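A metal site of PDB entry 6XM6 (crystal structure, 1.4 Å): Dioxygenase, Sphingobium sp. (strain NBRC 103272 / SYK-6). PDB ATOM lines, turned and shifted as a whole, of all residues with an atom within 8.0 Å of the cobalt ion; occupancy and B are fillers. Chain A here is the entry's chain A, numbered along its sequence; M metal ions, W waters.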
ATOM      1  N   PHE A  59       4.061  14.074  -8.447  1.00  0.00           N
ATOM      2  CA  PHE A  59       3.180  14.350  -9.547  1.00  0.00           C
ATOM      3  C   PHE A  59       3.380  13.384 -10.715  1.00  0.00           C
ATOM      4  O   PHE A  59       2.678  13.538 -11.726  1.00  0.00           O
ATOM      5  CB  PHE A  59       3.415  15.775 -10.067  1.00  0.00           C
ATOM      6  CG  PHE A  59       2.783  16.860  -9.247  1.00  0.00           C
ATOM      7  CD1 PHE A  59       2.103  16.612  -8.049  1.00  0.00           C
ATOM      8  CD2 PHE A  59       2.865  18.176  -9.695  1.00  0.00           C
ATOM      9  CE1 PHE A  59       1.547  17.652  -7.309  1.00  0.00           C
ATOM     10  CE2 PHE A  59       2.281  19.216  -8.964  1.00  0.00           C
ATOM     11  CZ  PHE A  59       1.635  18.962  -7.794  1.00  0.00           C
ATOM     12  N   THR A 121      -4.357  13.271 -12.570  1.00  0.00           N
ATOM     13  CA  THR A 121      -4.657  14.562 -11.948  1.00  0.00           C
ATOM     14  C   THR A 121      -6.131  14.772 -11.665  1.00  0.00           C
ATOM     15  O   THR A 121      -6.453  15.476 -10.699  1.00  0.00           O
ATOM     16  CB  THR A 121      -4.114  15.683 -12.848  1.00  0.00           C
ATOM     17  OG1 THR A 121      -2.685  15.502 -12.987  1.00  0.00           O
ATOM     18  CG2 THR A 121      -4.302  17.083 -12.301  1.00  0.00           C
ATOM     19  N   ASN A 122      -7.035  14.230 -12.478  1.00  0.00           N
ATOM     20  CA  ASN A 122      -8.449  14.327 -12.172  1.00  0.00           C
ATOM     21  C   ASN A 122      -9.156  13.064 -12.614  1.00  0.00           C
ATOM     22  O   ASN A 122      -8.717  12.365 -13.534  1.00  0.00           O
ATOM     23  CB  ASN A 122      -9.043  15.556 -12.877  1.00  0.00           C
ATOM     24  CG  ASN A 122     -10.252  16.123 -12.193  1.00  0.00           C
ATOM     25  OD1 ASN A 122     -10.952  15.458 -11.421  1.00  0.00           O
ATOM     26  ND2 ASN A 122     -10.528  17.382 -12.465  1.00  0.00           N
ATOM     27  N   GLU A 135      -2.588  16.895 -18.033  1.00  0.00           N
ATOM     28  CA  GLU A 135      -2.593  18.059 -18.914  1.00  0.00           C
ATOM     29  C   GLU A 135      -1.523  18.029 -20.008  1.00  0.00           C
ATOM     30  O   GLU A 135      -1.462  18.992 -20.764  1.00  0.00           O
ATOM     31  CB  GLU A 135      -2.440  19.304 -18.040  1.00  0.00           C
ATOM     32  CG  GLU A 135      -1.085  19.474 -17.391  1.00  0.00           C
ATOM     33  CD  GLU A 135      -1.180  20.359 -16.176  1.00  0.00           C
ATOM     34  OE1 GLU A 135      -1.957  20.070 -15.252  1.00  0.00           O
ATOM     35  OE2 GLU A 135      -0.416  21.312 -16.079  1.00  0.00           O
ATOM     36  N   ALA A 166      -6.529  19.017 -17.176  1.00  0.00           N
ATOM     37  CA  ALA A 166      -7.068  18.195 -16.092  1.00  0.00           C
ATOM     38  C   ALA A 166      -8.013  18.986 -15.201  1.00  0.00           C
ATOM     39  O   ALA A 166      -8.451  18.480 -14.174  1.00  0.00           O
ATOM     40  CB  ALA A 166      -5.950  17.560 -15.272  1.00  0.00           C
ATOM     41  N   HIS A 167      -8.394  20.215 -15.587  1.00  0.00           N
ATOM     42  CA  HIS A 167      -9.314  21.057 -14.843  1.00  0.00           C
ATOM     43  C   HIS A 167     -10.500  21.461 -15.712  1.00  0.00           C
ATOM     44  O   HIS A 167     -10.848  22.646 -15.800  1.00  0.00           O
ATOM     45  CB  HIS A 167      -8.557  22.263 -14.276  1.00  0.00           C
ATOM     46  CG  HIS A 167      -7.955  21.982 -12.955  1.00  0.00           C
ATOM     47  ND1 HIS A 167      -8.730  21.841 -11.821  1.00  0.00           N
ATOM     48  CD2 HIS A 167      -6.688  21.696 -12.578  1.00  0.00           C
ATOM     49  CE1 HIS A 167      -7.951  21.519 -10.794  1.00  0.00           C
ATOM     50  NE2 HIS A 167      -6.711  21.421 -11.230  1.00  0.00           N
ATOM     51  N   MET A 216       3.194  26.661 -16.747  1.00  0.00           N
ATOM     52  CA  MET A 216       2.197  25.688 -16.321  1.00  0.00           C
ATOM     53  C   MET A 216       0.824  26.344 -16.283  1.00  0.00           C
ATOM     54  O   MET A 216       0.525  27.120 -15.376  1.00  0.00           O
ATOM     55  CB  MET A 216       2.569  25.158 -14.944  1.00  0.00           C
ATOM     56  CG  MET A 216       1.733  23.984 -14.615  1.00  0.00           C
ATOM     57  SD  MET A 216       1.653  23.504 -12.880  1.00  0.00           S
ATOM     58  CE  MET A 216       3.336  23.067 -12.585  1.00  0.00           C
ATOM     59  N   HIS A 218      -2.217  25.235 -15.539  1.00  0.00           N
ATOM     60  CA  HIS A 218      -2.834  24.082 -14.880  1.00  0.00           C
ATOM     61  C   HIS A 218      -4.332  24.233 -14.751  1.00  0.00           C
ATOM     62  O   HIS A 218      -5.076  23.262 -14.900  1.00  0.00           O
ATOM     63  CB  HIS A 218      -2.180  23.896 -13.497  1.00  0.00           C
ATOM     64  CG  HIS A 218      -2.737  22.780 -12.690  1.00  0.00           C
ATOM     65  ND1 HIS A 218      -2.538  21.464 -13.001  1.00  0.00           N
ATOM     66  CD2 HIS A 218      -3.453  22.819 -11.552  1.00  0.00           C
ATOM     67  CE1 HIS A 218      -3.178  20.722 -12.100  1.00  0.00           C
ATOM     68  NE2 HIS A 218      -3.745  21.520 -11.212  1.00  0.00           N
ATOM     69  N   ASP A 219      -4.807  25.434 -14.474  1.00  0.00           N
ATOM     70  CA  ASP A 219      -6.207  25.665 -14.203  1.00  0.00           C
ATOM     71  C   ASP A 219      -6.570  26.990 -14.867  1.00  0.00           C
ATOM     72  O   ASP A 219      -5.719  27.647 -15.505  1.00  0.00           O
ATOM     73  CB  ASP A 219      -6.472  25.646 -12.670  1.00  0.00           C
ATOM     74  CG  ASP A 219      -7.918  25.396 -12.277  1.00  0.00           C
ATOM     75  OD1 ASP A 219      -8.789  25.274 -13.151  1.00  0.00           O
ATOM     76  OD2 ASP A 219      -8.094  25.302 -11.035  1.00  0.00           O
ATOM     77  N   SER A 283      -2.421  28.883  -8.640  1.00  0.00           N
ATOM     78  CA  SER A 283      -2.620  27.687  -9.453  1.00  0.00           C
ATOM     79  C   SER A 283      -4.094  27.436  -9.694  1.00  0.00           C
ATOM     80  O   SER A 283      -4.520  27.440 -10.849  1.00  0.00           O
ATOM     81  CB  SER A 283      -1.988  26.499  -8.738  1.00  0.00           C
ATOM     82  OG  SER A 283      -2.221  25.290  -9.441  1.00  0.00           O
ATOM     83  N   HIS A 284      -4.869  27.214  -8.644  1.00  0.00           N
ATOM     84  CA  HIS A 284      -6.240  26.789  -8.818  1.00  0.00           C
ATOM     85  C   HIS A 284      -7.226  27.948  -8.820  1.00  0.00           C
ATOM     86  O   HIS A 284      -6.965  29.024  -8.300  1.00  0.00           O
ATOM     87  CB  HIS A 284      -6.635  25.841  -7.699  1.00  0.00           C
ATOM     88  CG  HIS A 284      -6.022  24.488  -7.887  1.00  0.00           C
ATOM     89  ND1 HIS A 284      -5.235  23.887  -6.924  1.00  0.00           N
ATOM     90  CD2 HIS A 284      -6.077  23.638  -8.943  1.00  0.00           C
ATOM     91  CE1 HIS A 284      -4.849  22.707  -7.399  1.00  0.00           C
ATOM     92  NE2 HIS A 284      -5.302  22.555  -8.624  1.00  0.00           N
ATOM     93  N   VAL A 285      -8.381  27.695  -9.422  1.00  0.00           N
ATOM     94  CA  VAL A 285      -9.482  28.620  -9.521  1.00  0.00           C
ATOM     95  C   VAL A 285     -10.657  28.076  -8.720  1.00  0.00           C
ATOM     96  O   VAL A 285     -11.181  26.996  -9.003  1.00  0.00           O
ATOM     97  CB  VAL A 285      -9.873  28.842 -10.983  1.00  0.00           C
ATOM     98  CG1 VAL A 285     -11.118  29.701 -11.061  1.00  0.00           C
ATOM     99  CG2 VAL A 285      -8.747  29.492 -11.736  1.00  0.00           C
ATOM    100  N   PHE A 307       5.530  25.093  -5.358  1.00  0.00           N
ATOM    101  CA  PHE A 307       5.988  23.765  -5.749  1.00  0.00           C
ATOM    102  C   PHE A 307       7.463  23.617  -5.412  1.00  0.00           C
ATOM    103  O   PHE A 307       8.319  24.011  -6.220  1.00  0.00           O
ATOM    104  CB  PHE A 307       5.785  23.562  -7.263  1.00  0.00           C
ATOM    105  CG  PHE A 307       4.369  23.695  -7.733  1.00  0.00           C
ATOM    106  CD1 PHE A 307       3.348  22.992  -7.131  1.00  0.00           C
ATOM    107  CD2 PHE A 307       4.095  24.459  -8.858  1.00  0.00           C
ATOM    108  CE1 PHE A 307       2.063  23.089  -7.603  1.00  0.00           C
ATOM    109  CE2 PHE A 307       2.827  24.545  -9.345  1.00  0.00           C
ATOM    110  CZ  PHE A 307       1.805  23.869  -8.731  1.00  0.00           C
ATOM    111  N   GLU A 353      -5.965  25.713   0.028  1.00  0.00           N
ATOM    112  CA  GLU A 353      -5.851  25.358  -1.368  1.00  0.00           C
ATOM    113  C   GLU A 353      -6.969  24.381  -1.700  1.00  0.00           C
ATOM    114  O   GLU A 353      -7.909  24.190  -0.910  1.00  0.00           O
ATOM    115  CB  GLU A 353      -4.495  24.732  -1.683  1.00  0.00           C
ATOM    116  CG  GLU A 353      -3.641  25.613  -2.566  1.00  0.00           C
ATOM    117  CD  GLU A 353      -4.031  25.572  -4.012  1.00  0.00           C
ATOM    118  OE1 GLU A 353      -3.361  26.251  -4.813  1.00  0.00           O
ATOM    119  OE2 GLU A 353      -4.895  24.798  -4.427  1.00  0.00           O
ATOM    120  N   PHE A 354      -6.893  23.751  -2.869  1.00  0.00           N
ATOM    121  CA  PHE A 354      -7.944  22.839  -3.328  1.00  0.00           C
ATOM    122  C   PHE A 354      -9.328  23.476  -3.201  1.00  0.00           C
ATOM    123  O   PHE A 354     -10.247  22.899  -2.627  1.00  0.00           O
ATOM    124  CB  PHE A 354      -7.884  21.507  -2.590  1.00  0.00           C
ATOM    125  CG  PHE A 354      -6.871  20.500  -3.093  1.00  0.00           C
ATOM    126  CD1 PHE A 354      -6.931  19.994  -4.362  1.00  0.00           C
ATOM    127  CD2 PHE A 354      -5.973  19.948  -2.200  1.00  0.00           C
ATOM    128  CE1 PHE A 354      -6.064  19.016  -4.780  1.00  0.00           C
ATOM    129  CE2 PHE A 354      -5.093  18.940  -2.621  1.00  0.00           C
ATOM    130  CZ  PHE A 354      -5.144  18.489  -3.909  1.00  0.00           C
ATOM    131  N   PRO A 355      -9.524  24.639  -3.811  1.00  0.00           N
ATOM    132  CA  PRO A 355     -10.819  25.304  -3.744  1.00  0.00           C
ATOM    133  C   PRO A 355     -11.875  24.600  -4.559  1.00  0.00           C
ATOM    134  O   PRO A 355     -11.623  24.123  -5.661  1.00  0.00           O
ATOM    135  CB  PRO A 355     -10.538  26.667  -4.355  1.00  0.00           C
ATOM    136  CG  PRO A 355      -9.470  26.380  -5.359  1.00  0.00           C
ATOM    137  CD  PRO A 355      -8.571  25.319  -4.710  1.00  0.00           C
ATOM    138  N   GLU A 418      -8.868  16.649  -1.131  1.00  0.00           N
ATOM    139  CA  GLU A 418      -9.745  17.657  -1.729  1.00  0.00           C
ATOM    140  C   GLU A 418     -11.221  17.325  -1.452  1.00  0.00           C
ATOM    141  O   GLU A 418     -11.666  16.196  -1.715  1.00  0.00           O
ATOM    142  CB  GLU A 418      -9.507  17.748  -3.246  1.00  0.00           C
ATOM    143  CG  GLU A 418     -10.422  18.750  -3.921  1.00  0.00           C
ATOM    144  CD  GLU A 418     -10.447  18.559  -5.410  1.00  0.00           C
ATOM    145  OE1 GLU A 418     -10.731  17.489  -5.945  1.00  0.00           O
ATOM    146  OE2 GLU A 418     -10.134  19.582  -6.093  1.00  0.00           O
ATOM    147  N   LEU A 475      -5.161  13.905  -6.018  1.00  0.00           N
ATOM    148  CA  LEU A 475      -5.354  15.152  -6.744  1.00  0.00           C
ATOM    149  C   LEU A 475      -6.856  15.399  -6.795  1.00  0.00           C
ATOM    150  O   LEU A 475      -7.453  15.540  -5.732  1.00  0.00           O
ATOM    151  CB  LEU A 475      -4.594  15.172  -8.056  1.00  0.00           C
ATOM    152  CG  LEU A 475      -3.087  15.296  -7.782  1.00  0.00           C
ATOM    153  CD1 LEU A 475      -2.229  15.006  -9.020  1.00  0.00           C
ATOM    154  CD2 LEU A 475      -2.753  16.726  -7.252  1.00  0.00           C
ATOM    155  N   HIS A 476      -7.477  15.487  -7.939  1.00  0.00           N
ATOM    156  CA  HIS A 476      -8.841  15.998  -7.994  1.00  0.00           C
ATOM    157  C   HIS A 476      -9.865  14.888  -8.138  1.00  0.00           C
ATOM    158  O   HIS A 476      -9.567  13.774  -8.574  1.00  0.00           O
ATOM    159  CB  HIS A 476      -8.980  17.051  -9.120  1.00  0.00           C
ATOM    160  CG  HIS A 476      -8.048  18.192  -8.944  1.00  0.00           C
ATOM    161  ND1 HIS A 476      -8.191  19.129  -7.962  1.00  0.00           N
ATOM    162  CD2 HIS A 476      -6.868  18.466  -9.542  1.00  0.00           C
ATOM    163  CE1 HIS A 476      -7.173  19.965  -7.977  1.00  0.00           C
ATOM    164  NE2 HIS A 476      -6.362  19.623  -8.968  1.00  0.00           N
HETATM  165 CO    CO M   1      -5.135  20.947  -9.880  1.00  0.00          CO
HETATM  166  O   HOH W   1      -3.497  20.099  -8.748  1.00  0.00           O
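Of the 19 residues printed, 4 come within 4 Å of the cobalt ion.
The cobalt ion is bound by NE2 of His 218, NE2 of His 476, NE2 of His 284, NE2 of His 167 and water W1.
ND1 of His 284 is in hydrogen-bond range of OE2 of Glu 353. A ring nitrogen (ND1) of His 476 is in hydrogen-bond range of the side-chain carboxylate (OE2) of Glu 418, at 2.7 Å. N of His 476 lies within hydrogen-bond range of O of Thr 121. The side-chain carboxylate (OE1) of Glu 135 lies within hydrogen-bond range of a ring nitrogen (ND1) of His 218, 2.7 Å away.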
